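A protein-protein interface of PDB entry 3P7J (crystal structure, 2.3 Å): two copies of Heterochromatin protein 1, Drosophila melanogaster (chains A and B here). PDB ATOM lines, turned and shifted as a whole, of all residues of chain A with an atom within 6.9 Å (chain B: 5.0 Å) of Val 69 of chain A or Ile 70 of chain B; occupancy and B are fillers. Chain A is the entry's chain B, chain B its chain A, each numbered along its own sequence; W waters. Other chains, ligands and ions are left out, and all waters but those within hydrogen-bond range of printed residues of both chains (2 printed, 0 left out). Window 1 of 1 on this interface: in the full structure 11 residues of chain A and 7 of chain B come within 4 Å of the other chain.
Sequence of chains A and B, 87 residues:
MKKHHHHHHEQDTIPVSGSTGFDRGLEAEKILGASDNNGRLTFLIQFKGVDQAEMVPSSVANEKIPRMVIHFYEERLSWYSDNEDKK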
ATOM      1  N   ILE A  31     -12.258  -3.671  -9.794  1.00  0.00           N
ATOM      2  CA  ILE A  31     -12.469  -2.297  -9.399  1.00  0.00           C
ATOM      3  C   ILE A  31     -11.284  -1.982  -8.496  1.00  0.00           C
ATOM      4  O   ILE A  31     -11.073  -2.661  -7.496  1.00  0.00           O
ATOM      5  CB  ILE A  31     -13.759  -2.082  -8.605  1.00  0.00           C
ATOM      6  CG1 ILE A  31     -14.981  -2.329  -9.488  1.00  0.00           C
ATOM      7  CG2 ILE A  31     -13.807  -0.645  -8.079  1.00  0.00           C
ATOM      8  CD1 ILE A  31     -16.333  -2.385  -8.697  1.00  0.00           C
ATOM      9  N   PHE A  43     -15.640   5.185 -10.299  1.00  0.00           N
ATOM     10  CA  PHE A  43     -14.797   4.006 -10.032  1.00  0.00           C
ATOM     11  C   PHE A  43     -13.581   3.974 -10.945  1.00  0.00           C
ATOM     12  O   PHE A  43     -13.648   4.380 -12.092  1.00  0.00           O
ATOM     13  CB  PHE A  43     -15.581   2.729 -10.311  1.00  0.00           C
ATOM     14  CG  PHE A  43     -16.537   2.394  -9.255  1.00  0.00           C
ATOM     15  CD1 PHE A  43     -16.087   2.141  -7.977  1.00  0.00           C
ATOM     16  CD2 PHE A  43     -17.896   2.362  -9.520  1.00  0.00           C
ATOM     17  CE1 PHE A  43     -16.947   1.839  -6.983  1.00  0.00           C
ATOM     18  CE2 PHE A  43     -18.795   2.042  -8.503  1.00  0.00           C
ATOM     19  CZ  PHE A  43     -18.311   1.782  -7.239  1.00  0.00           C
ATOM     20  N   ILE A  45     -11.555   1.315 -12.888  1.00  0.00           N
ATOM     21  CA  ILE A  45     -11.787  -0.055 -13.302  1.00  0.00           C
ATOM     22  C   ILE A  45     -10.723  -0.650 -14.235  1.00  0.00           C
ATOM     23  O   ILE A  45     -10.444  -0.113 -15.303  1.00  0.00           O
ATOM     24  CB  ILE A  45     -13.183  -0.165 -13.975  1.00  0.00           C
ATOM     25  CG1 ILE A  45     -14.250   0.268 -12.951  1.00  0.00           C
ATOM     26  CG2 ILE A  45     -13.416  -1.598 -14.506  1.00  0.00           C
ATOM     27  CD1 ILE A  45     -15.654  -0.110 -13.283  1.00  0.00           C
ATOM     28  N   SER A  58     -20.120   5.687 -11.299  1.00  0.00           N
ATOM     29  CA  SER A  58     -20.864   4.655 -10.602  1.00  0.00           C
ATOM     30  C   SER A  58     -22.175   4.311 -11.308  1.00  0.00           C
ATOM     31  O   SER A  58     -22.566   3.157 -11.306  1.00  0.00           O
ATOM     32  CB  SER A  58     -21.134   5.049  -9.148  1.00  0.00           C
ATOM     33  OG  SER A  58     -21.725   6.329  -9.066  1.00  0.00           O
ATOM     34  N   VAL A  60     -22.926   3.971 -14.428  1.00  0.00           N
ATOM     35  CA  VAL A  60     -22.628   2.910 -15.405  1.00  0.00           C
ATOM     36  C   VAL A  60     -22.251   1.603 -14.682  1.00  0.00           C
ATOM     37  O   VAL A  60     -22.770   0.517 -15.040  1.00  0.00           O
ATOM     38  CB  VAL A  60     -21.534   3.335 -16.449  1.00  0.00           C
ATOM     39  CG1 VAL A  60     -21.312   2.243 -17.513  1.00  0.00           C
ATOM     40  CG2 VAL A  60     -21.945   4.662 -17.146  1.00  0.00           C
ATOM     41  N   ALA A  61     -21.380   1.680 -13.669  1.00  0.00           N
ATOM     42  CA  ALA A  61     -20.839   0.416 -13.066  1.00  0.00           C
ATOM     43  C   ALA A  61     -21.958  -0.314 -12.339  1.00  0.00           C
ATOM     44  O   ALA A  61     -22.111  -1.551 -12.493  1.00  0.00           O
ATOM     45  CB  ALA A  61     -19.600   0.648 -12.177  1.00  0.00           C
ATOM     46  N   ASN A  62     -22.793   0.446 -11.625  1.00  0.00           N
ATOM     47  CA  ASN A  62     -23.921  -0.137 -10.895  1.00  0.00           C
ATOM     48  C   ASN A  62     -24.844  -0.956 -11.809  1.00  0.00           C
ATOM     49  O   ASN A  62     -25.399  -1.952 -11.403  1.00  0.00           O
ATOM     50  CB  ASN A  62     -24.756   0.944 -10.199  1.00  0.00           C
ATOM     51  CG  ASN A  62     -23.990   1.664  -9.109  1.00  0.00           C
ATOM     52  OD1 ASN A  62     -22.883   1.249  -8.758  1.00  0.00           O
ATOM     53  ND2 ASN A  62     -24.575   2.748  -8.562  1.00  0.00           N
ATOM     54  N   GLU A  63     -24.981  -0.523 -13.055  1.00  0.00           N
ATOM     55  CA  GLU A  63     -25.908  -1.166 -13.991  1.00  0.00           C
ATOM     56  C   GLU A  63     -25.285  -2.367 -14.683  1.00  0.00           C
ATOM     57  O   GLU A  63     -25.964  -3.355 -14.951  1.00  0.00           O
ATOM     58  CB  GLU A  63     -26.363  -0.162 -15.058  1.00  0.00           C
ATOM     59  CG  GLU A  63     -27.811  -0.360 -15.496  1.00  0.00           C
ATOM     60  CD  GLU A  63     -28.825  -0.002 -14.372  1.00  0.00           C
ATOM     61  OE1 GLU A  63     -28.455   0.766 -13.431  1.00  0.00           O
ATOM     62  OE2 GLU A  63     -29.984  -0.494 -14.436  1.00  0.00           O
ATOM     63  N   LYS A  64     -23.992  -2.259 -14.988  1.00  0.00           N
ATOM     64  CA  LYS A  64     -23.288  -3.263 -15.805  1.00  0.00           C
ATOM     65  C   LYS A  64     -22.681  -4.396 -14.990  1.00  0.00           C
ATOM     66  O   LYS A  64     -22.685  -5.549 -15.430  1.00  0.00           O
ATOM     67  CB  LYS A  64     -22.148  -2.607 -16.596  1.00  0.00           C
ATOM     68  CG  LYS A  64     -22.598  -1.648 -17.721  1.00  0.00           C
ATOM     69  CD  LYS A  64     -23.045  -2.431 -18.974  1.00  0.00           C
ATOM     70  CE  LYS A  64     -23.621  -1.492 -20.019  1.00  0.00           C
ATOM     71  NZ  LYS A  64     -23.877  -2.244 -21.269  1.00  0.00           N
ATOM     72  N   ILE A  65     -22.121  -4.047 -13.839  1.00  0.00           N
ATOM     73  CA  ILE A  65     -21.395  -4.988 -12.999  1.00  0.00           C
ATOM     74  C   ILE A  65     -21.806  -4.888 -11.520  1.00  0.00           C
ATOM     75  O   ILE A  65     -20.986  -4.635 -10.636  1.00  0.00           O
ATOM     76  CB  ILE A  65     -19.875  -4.847 -13.188  1.00  0.00           C
ATOM     77  CG1 ILE A  65     -19.400  -3.403 -12.925  1.00  0.00           C
ATOM     78  CG2 ILE A  65     -19.485  -5.417 -14.602  1.00  0.00           C
ATOM     79  CD1 ILE A  65     -17.835  -3.263 -12.773  1.00  0.00           C
ATOM     80  N   PRO A  66     -23.083  -5.128 -11.252  1.00  0.00           N
ATOM     81  CA  PRO A  66     -23.520  -4.924  -9.873  1.00  0.00           C
ATOM     82  C   PRO A  66     -22.894  -5.929  -8.883  1.00  0.00           C
ATOM     83  O   PRO A  66     -22.676  -5.586  -7.742  1.00  0.00           O
ATOM     84  CB  PRO A  66     -25.054  -5.088  -9.957  1.00  0.00           C
ATOM     85  CG  PRO A  66     -25.290  -5.974 -11.258  1.00  0.00           C
ATOM     86  CD  PRO A  66     -24.183  -5.478 -12.179  1.00  0.00           C
ATOM     87  N   ARG A  67     -22.644  -7.164  -9.315  1.00  0.00           N
ATOM     88  CA  ARG A  67     -22.042  -8.184  -8.437  1.00  0.00           C
ATOM     89  C   ARG A  67     -20.631  -7.764  -8.053  1.00  0.00           C
ATOM     90  O   ARG A  67     -20.202  -7.941  -6.914  1.00  0.00           O
ATOM     91  CB  ARG A  67     -22.024  -9.562  -9.122  1.00  0.00           C
ATOM     92  CG  ARG A  67     -23.431 -10.191  -9.189  1.00  0.00           C
ATOM     93  CD  ARG A  67     -23.495 -11.389 -10.179  1.00  0.00           C
ATOM     94  NE  ARG A  67     -22.470 -12.386  -9.827  1.00  0.00           N
ATOM     95  CZ  ARG A  67     -22.637 -13.392  -8.970  1.00  0.00           C
ATOM     96  NH1 ARG A  67     -23.803 -13.602  -8.370  1.00  0.00           N
ATOM     97  NH2 ARG A  67     -21.626 -14.188  -8.707  1.00  0.00           N
ATOM     98  N   MET A  68     -19.910  -7.196  -9.013  1.00  0.00           N
ATOM     99  CA  MET A  68     -18.534  -6.769  -8.743  1.00  0.00           C
ATOM    100  C   MET A  68     -18.518  -5.469  -7.904  1.00  0.00           C
ATOM    101  O   MET A  68     -17.609  -5.285  -7.095  1.00  0.00           O
ATOM    102  CB  MET A  68     -17.762  -6.602 -10.057  1.00  0.00           C
ATOM    103  CG  MET A  68     -16.300  -6.175  -9.921  1.00  0.00           C
ATOM    104  SD  MET A  68     -15.447  -6.172 -11.531  1.00  0.00           S
ATOM    105  CE  MET A  68     -14.951  -7.930 -11.558  1.00  0.00           C
ATOM    106  N   VAL A  69     -19.513  -4.586  -8.126  1.00  0.00           N
ATOM    107  CA  VAL A  69     -19.691  -3.402  -7.298  1.00  0.00           C
ATOM    108  C   VAL A  69     -19.964  -3.781  -5.830  1.00  0.00           C
ATOM    109  O   VAL A  69     -19.289  -3.307  -4.898  1.00  0.00           O
ATOM    110  CB  VAL A  69     -20.747  -2.445  -7.909  1.00  0.00           C
ATOM    111  CG1 VAL A  69     -21.187  -1.286  -6.906  1.00  0.00           C
ATOM    112  CG2 VAL A  69     -20.189  -1.843  -9.215  1.00  0.00           C
ATOM    113  N   ILE A  70     -20.926  -4.662  -5.627  1.00  0.00           N
ATOM    114  CA  ILE A  70     -21.289  -5.079  -4.306  1.00  0.00           C
ATOM    115  C   ILE A  70     -20.106  -5.736  -3.570  1.00  0.00           C
ATOM    116  O   ILE A  70     -19.803  -5.415  -2.402  1.00  0.00           O
ATOM    117  CB  ILE A  70     -22.511  -6.037  -4.371  1.00  0.00           C
ATOM    118  CG1 ILE A  70     -23.772  -5.223  -4.719  1.00  0.00           C
ATOM    119  CG2 ILE A  70     -22.660  -6.808  -3.035  1.00  0.00           C
ATOM    120  CD1 ILE A  70     -25.051  -6.069  -4.841  1.00  0.00           C
ATOM    121  N   HIS A  71     -19.449  -6.653  -4.267  1.00  0.00           N
ATOM    122  CA  HIS A  71     -18.262  -7.295  -3.722  1.00  0.00           C
ATOM    123  C   HIS A  71     -17.185  -6.283  -3.327  1.00  0.00           C
ATOM    124  O   HIS A  71     -16.531  -6.453  -2.311  1.00  0.00           O
ATOM    125  CB  HIS A  71     -17.718  -8.255  -4.762  1.00  0.00           C
ATOM    126  CG  HIS A  71     -16.816  -9.292  -4.207  1.00  0.00           C
ATOM    127  ND1 HIS A  71     -17.267 -10.317  -3.394  1.00  0.00           N
ATOM    128  CD2 HIS A  71     -15.489  -9.482  -4.362  1.00  0.00           C
ATOM    129  CE1 HIS A  71     -16.244 -11.079  -3.059  1.00  0.00           C
ATOM    130  NE2 HIS A  71     -15.156 -10.593  -3.627  1.00  0.00           N
ATOM    131  N   PHE A  72     -16.965  -5.260  -4.155  1.00  0.00           N
ATOM    132  CA  PHE A  72     -15.972  -4.253  -3.846  1.00  0.00           C
ATOM    133  C   PHE A  72     -16.344  -3.582  -2.505  1.00  0.00           C
ATOM    134  O   PHE A  72     -15.486  -3.342  -1.662  1.00  0.00           O
ATOM    135  CB  PHE A  72     -15.927  -3.189  -4.940  1.00  0.00           C
ATOM    136  CG  PHE A  72     -15.128  -1.930  -4.563  1.00  0.00           C
ATOM    137  CD1 PHE A  72     -13.736  -1.945  -4.595  1.00  0.00           C
ATOM    138  CD2 PHE A  72     -15.779  -0.756  -4.213  1.00  0.00           C
ATOM    139  CE1 PHE A  72     -12.977  -0.794  -4.276  1.00  0.00           C
ATOM    140  CE2 PHE A  72     -15.059   0.411  -3.886  1.00  0.00           C
ATOM    141  CZ  PHE A  72     -13.646   0.393  -3.900  1.00  0.00           C
ATOM    142  N   TYR A  73     -17.619  -3.250  -2.351  1.00  0.00           N
ATOM    143  CA  TYR A  73     -18.084  -2.585  -1.131  1.00  0.00           C
ATOM    144  C   TYR A  73     -18.022  -3.487   0.111  1.00  0.00           C
ATOM    145  O   TYR A  73     -17.644  -3.039   1.218  1.00  0.00           O
ATOM    146  CB  TYR A  73     -19.510  -2.097  -1.302  1.00  0.00           C
ATOM    147  CG  TYR A  73     -19.637  -0.828  -2.117  1.00  0.00           C
ATOM    148  CD1 TYR A  73     -18.943   0.323  -1.771  1.00  0.00           C
ATOM    149  CD2 TYR A  73     -20.534  -0.755  -3.194  1.00  0.00           C
ATOM    150  CE1 TYR A  73     -19.099   1.526  -2.514  1.00  0.00           C
ATOM    151  CE2 TYR A  73     -20.691   0.421  -3.934  1.00  0.00           C
ATOM    152  CZ  TYR A  73     -19.972   1.554  -3.587  1.00  0.00           C
ATOM    153  OH  TYR A  73     -20.131   2.703  -4.310  1.00  0.00           O
ATOM    154  N   GLU A  74     -18.383  -4.756  -0.065  1.00  0.00           N
ATOM    155  CA  GLU A  74     -18.260  -5.704   1.039  1.00  0.00           C
ATOM    156  C   GLU A  74     -16.849  -5.714   1.556  1.00  0.00           C
ATOM    157  O   GLU A  74     -16.646  -5.538   2.755  1.00  0.00           O
ATOM    158  CB  GLU A  74     -18.671  -7.089   0.610  1.00  0.00           C
ATOM    159  CG  GLU A  74     -20.172  -7.220   0.545  1.00  0.00           C
ATOM    160  CD  GLU A  74     -20.596  -8.569   0.024  1.00  0.00           C
ATOM    161  OE1 GLU A  74     -21.800  -8.872   0.062  1.00  0.00           O
ATOM    162  OE2 GLU A  74     -19.718  -9.345  -0.410  1.00  0.00           O
ATOM    163  N   PRO B  66     -30.345  -5.797  -5.256  1.00  0.00           N
ATOM    164  CA  PRO B  66     -28.990  -5.294  -5.509  1.00  0.00           C
ATOM    165  C   PRO B  66     -28.864  -3.770  -5.625  1.00  0.00           C
ATOM    166  O   PRO B  66     -27.846  -3.226  -5.172  1.00  0.00           O
ATOM    167  CB  PRO B  66     -28.593  -5.959  -6.857  1.00  0.00           C
ATOM    168  CG  PRO B  66     -29.881  -6.406  -7.493  1.00  0.00           C
ATOM    169  CD  PRO B  66     -30.780  -6.748  -6.306  1.00  0.00           C
ATOM    170  N   ARG B  67     -29.860  -3.106  -6.248  1.00  0.00           N
ATOM    171  CA  ARG B  67     -29.829  -1.617  -6.411  1.00  0.00           C
ATOM    172  C   ARG B  67     -29.907  -0.940  -5.032  1.00  0.00           C
ATOM    173  O   ARG B  67     -29.178   0.027  -4.744  1.00  0.00           O
ATOM    174  CB  ARG B  67     -30.959  -1.105  -7.284  1.00  0.00           C
ATOM    175  CG  ARG B  67     -30.762  -1.314  -8.755  1.00  0.00           C
ATOM    176  CD  ARG B  67     -31.596  -0.272  -9.537  1.00  0.00           C
ATOM    177  NE  ARG B  67     -31.742  -0.598 -10.950  1.00  0.00           N
ATOM    178  CZ  ARG B  67     -32.752  -1.302 -11.462  1.00  0.00           C
ATOM    179  NH1 ARG B  67     -32.796  -1.537 -12.772  1.00  0.00           N
ATOM    180  NH2 ARG B  67     -33.724  -1.773 -10.670  1.00  0.00           N
ATOM    181  N   MET B  68     -30.761  -1.491  -4.169  1.00  0.00           N
ATOM    182  CA  MET B  68     -30.940  -0.970  -2.807  1.00  0.00           C
ATOM    183  C   MET B  68     -29.657  -1.222  -1.979  1.00  0.00           C
ATOM    184  O   MET B  68     -29.217  -0.369  -1.229  1.00  0.00           O
ATOM    185  CB  MET B  68     -32.189  -1.570  -2.178  1.00  0.00           C
ATOM    186  CG  MET B  68     -32.698  -0.771  -0.988  1.00  0.00           C
ATOM    187  SD  MET B  68     -34.223  -1.355  -0.237  1.00  0.00           S
ATOM    188  CE  MET B  68     -35.400  -1.040  -1.574  1.00  0.00           C
ATOM    189  N   VAL B  69     -29.033  -2.389  -2.153  1.00  0.00           N
ATOM    190  CA  VAL B  69     -27.773  -2.693  -1.431  1.00  0.00           C
ATOM    191  C   VAL B  69     -26.679  -1.713  -1.883  1.00  0.00           C
ATOM    192  O   VAL B  69     -25.958  -1.122  -1.075  1.00  0.00           O
ATOM    193  CB  VAL B  69     -27.317  -4.160  -1.658  1.00  0.00           C
ATOM    194  CG1 VAL B  69     -25.838  -4.407  -1.185  1.00  0.00           C
ATOM    195  CG2 VAL B  69     -28.308  -5.156  -0.967  1.00  0.00           C
ATOM    196  N   ILE B  70     -26.563  -1.513  -3.186  1.00  0.00           N
ATOM    197  CA  ILE B  70     -25.536  -0.601  -3.686  1.00  0.00           C
ATOM    198  C   ILE B  70     -25.752   0.834  -3.177  1.00  0.00           C
ATOM    199  O   ILE B  70     -24.804   1.503  -2.793  1.00  0.00           O
ATOM    200  CB  ILE B  70     -25.496  -0.611  -5.228  1.00  0.00           C
ATOM    201  CG1 ILE B  70     -24.948  -1.971  -5.694  1.00  0.00           C
ATOM    202  CG2 ILE B  70     -24.638   0.561  -5.770  1.00  0.00           C
ATOM    203  CD1 ILE B  70     -24.880  -2.147  -7.200  1.00  0.00           C
ATOM    204  N   HIS B  71     -27.007   1.295  -3.236  1.00  0.00           N
ATOM    205  CA  HIS B  71     -27.367   2.637  -2.751  1.00  0.00           C
ATOM    206  C   HIS B  71     -27.055   2.801  -1.256  1.00  0.00           C
ATOM    207  O   HIS B  71     -26.555   3.844  -0.829  1.00  0.00           O
ATOM    208  CB  HIS B  71     -28.845   2.951  -3.003  1.00  0.00           C
ATOM    209  CG  HIS B  71     -29.253   4.303  -2.525  1.00  0.00           C
ATOM    210  ND1 HIS B  71     -30.275   4.495  -1.613  1.00  0.00           N
ATOM    211  CD2 HIS B  71     -28.764   5.539  -2.810  1.00  0.00           C
ATOM    212  CE1 HIS B  71     -30.406   5.791  -1.371  1.00  0.00           C
ATOM    213  NE2 HIS B  71     -29.502   6.443  -2.082  1.00  0.00           N
ATOM    214  N   PHE B  72     -27.264   1.734  -0.497  1.00  0.00           N
ATOM    215  CA  PHE B  72     -26.958   1.757   0.937  1.00  0.00           C
ATOM    216  C   PHE B  72     -25.476   1.935   1.155  1.00  0.00           C
ATOM    217  O   PHE B  72     -25.026   2.735   1.986  1.00  0.00           O
ATOM    218  CB  PHE B  72     -27.395   0.432   1.581  1.00  0.00           C
ATOM    219  CG  PHE B  72     -26.984   0.304   3.014  1.00  0.00           C
ATOM    220  CD1 PHE B  72     -27.739   0.903   4.020  1.00  0.00           C
ATOM    221  CD2 PHE B  72     -25.852  -0.441   3.365  1.00  0.00           C
ATOM    222  CE1 PHE B  72     -27.362   0.788   5.347  1.00  0.00           C
ATOM    223  CE2 PHE B  72     -25.451  -0.552   4.711  1.00  0.00           C
ATOM    224  CZ  PHE B  72     -26.199   0.057   5.694  1.00  0.00           C
ATOM    225  N   TYR B  73     -24.700   1.158   0.417  1.00  0.00           N
ATOM    226  CA  TYR B  73     -23.246   1.270   0.565  1.00  0.00           C
ATOM    227  C   TYR B  73     -22.712   2.601   0.066  1.00  0.00           C
ATOM    228  O   TYR B  73     -21.779   3.177   0.652  1.00  0.00           O
ATOM    229  CB  TYR B  73     -22.553   0.200  -0.222  1.00  0.00           C
ATOM    230  CG  TYR B  73     -22.592  -1.148   0.396  1.00  0.00           C
ATOM    231  CD1 TYR B  73     -22.135  -1.349   1.696  1.00  0.00           C
ATOM    232  CD2 TYR B  73     -23.016  -2.240  -0.350  1.00  0.00           C
ATOM    233  CE1 TYR B  73     -22.148  -2.585   2.244  1.00  0.00           C
ATOM    234  CE2 TYR B  73     -23.001  -3.496   0.185  1.00  0.00           C
ATOM    235  CZ  TYR B  73     -22.580  -3.661   1.489  1.00  0.00           C
ATOM    236  OH  TYR B  73     -22.573  -4.908   2.039  1.00  0.00           O
ATOM    237  N   GLU B  74     -23.284   3.053  -1.053  1.00  0.00           N
ATOM    238  CA  GLU B  74     -22.906   4.323  -1.669  1.00  0.00           C
ATOM    239  C   GLU B  74     -23.148   5.452  -0.723  1.00  0.00           C
ATOM    240  O   GLU B  74     -22.309   6.323  -0.581  1.00  0.00           O
ATOM    241  CB  GLU B  74     -23.778   4.617  -2.864  1.00  0.00           C
ATOM    242  CG  GLU B  74     -23.103   4.428  -4.156  1.00  0.00           C
ATOM    243  CD  GLU B  74     -24.069   4.556  -5.317  1.00  0.00           C
ATOM    244  OE1 GLU B  74     -25.287   4.778  -5.077  1.00  0.00           O
ATOM    245  OE2 GLU B  74     -23.608   4.421  -6.467  1.00  0.00           O
ATOM    246  N   GLU B  75     -24.317   5.443  -0.085  1.00  0.00           N
ATOM    247  CA  GLU B  75     -24.662   6.504   0.859  1.00  0.00           C
ATOM    248  C   GLU B  75     -23.806   6.417   2.150  1.00  0.00           C
ATOM    249  O   GLU B  75     -23.314   7.459   2.659  1.00  0.00           O
ATOM    250  CB  GLU B  75     -26.174   6.515   1.156  1.00  0.00           C
ATOM    251  CG  GLU B  75     -26.590   5.720   2.396  1.00  0.00           C
ATOM    252  CD  GLU B  75     -28.097   5.504   2.518  1.00  0.00           C
ATOM    253  OE1 GLU B  75     -28.831   6.521   2.653  1.00  0.00           O
ATOM    254  OE2 GLU B  75     -28.533   4.319   2.511  1.00  0.00           O
HETATM  255  O   HOH W   1     -23.588  -7.118   0.436  1.00  0.00           O
HETATM  256  O   HOH W   2     -21.900   2.519  -6.564  1.00  0.00           O
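Printed residues of chain B within 4 Å of Ser 58 of chain A: Glu 74. Ile 65 of chain A touches none of the printed residues of chain B. Arg 67 of chain A touches none of the printed residues of chain B. Of the printed residues of chain B, Ile 70 of chain A touches Ile 70. Of the printed residues of chain A, Ile 70 of chain B touches Asn 62, Val 69 and Ile 70. Of the printed residues of chain A, Tyr 73 of chain B touches Tyr 73 and Glu 74. The nearest printed residue of chain B that does not touch Val 69 of chain A is Tyr 73 of chain B (6.0 Å). The nearest printed residue of chain B that does not touch Glu 63 of chain A is Ile 70 of chain B (6.1 Å).
The side-chain carboxylate of Glu 74 of chain B lies within hydrogen-bond range of the side-chain amide nitrogen of Asn 62 of chain A, 2.9 Å away. The side-chain carboxylate (OE2) of Glu 63 of chain A lies within salt-bridge range of the guanidinium group (NH1) of Arg 67 of chain B (3.4 Å).
Printed residues of chain A that touch a printed residue of chain B: Ser 58, Asn 62, Glu 63, Val 69, Ile 70, Tyr 73 and Glu 74. Hydrophobic or aromatic side chains of chain A within 4 Å of the printed part of chain B: Val 69, Ile 70 and Tyr 73. Of the 10 printed residues of chain B, 4 touch a printed residue of chain A. Hydrophobic or aromatic side chains of chain B within 4 Å of the printed part of chain A: Ile 70 and Tyr 73. Among the printed residues, 9 pairs touch across the chains. Among the printed residues, Asp or Glu carboxylates within 4 Å of a Lys or Arg side-chain nitrogen of the other chain: Glu 63 of chain A with Arg 67 of chain B (3.4 Å).
Among the printed residues, merely in contact across the chains: Ser 58 of chain A with Glu 74 of chain B, Asn 62 of chain A with Ile 70 of chain B, Val 69 of chain A with Ile 70 of chain B, Ile 70 of chain A with Ile 70 of chain B, Tyr 73 of chain A with Tyr 73 of chain B, Tyr 73 of chain A with Glu 74 of chain B and Glu 74 of chain A with Tyr 73 of chain B.
Water W1 bridges the side-chain carboxylate (OE1) of Glu 74 of chain A (2.5 Å) and the side-chain hydroxyl (OH) of Tyr 73 of chain B (2.9 Å). Water W2 lies within hydrogen-bond range of OE2 of Glu 74 of chain B (2.6 Å), OD1 of Asn 62 of chain A (2.7 Å) and OH of Tyr 73 of chain A (2.9 Å).
O of Ser 58 of chain A lies close to OD1 of Asn 62 of chain A, at 3.2 Å.
Val 69 of chain A touches Ile 70 of chain B, but with the chains exchanged Ile 70 of chain A does not touch Val 69 of chain B (4.1 Å). Ile 70 of chain A touches its own counterpart, Ile 70 of chain B. Tyr 73 of chain A touches its own counterpart, Tyr 73 of chain B. Tyr 73 of chain A touches Glu 74 of chain B, and with the chains exchanged Glu 74 of chain A touches Tyr 73 of chain B. Of the 9 pairs that touch across the chains among the printed residues, 4 have their exchanged pair printed and touching as well.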
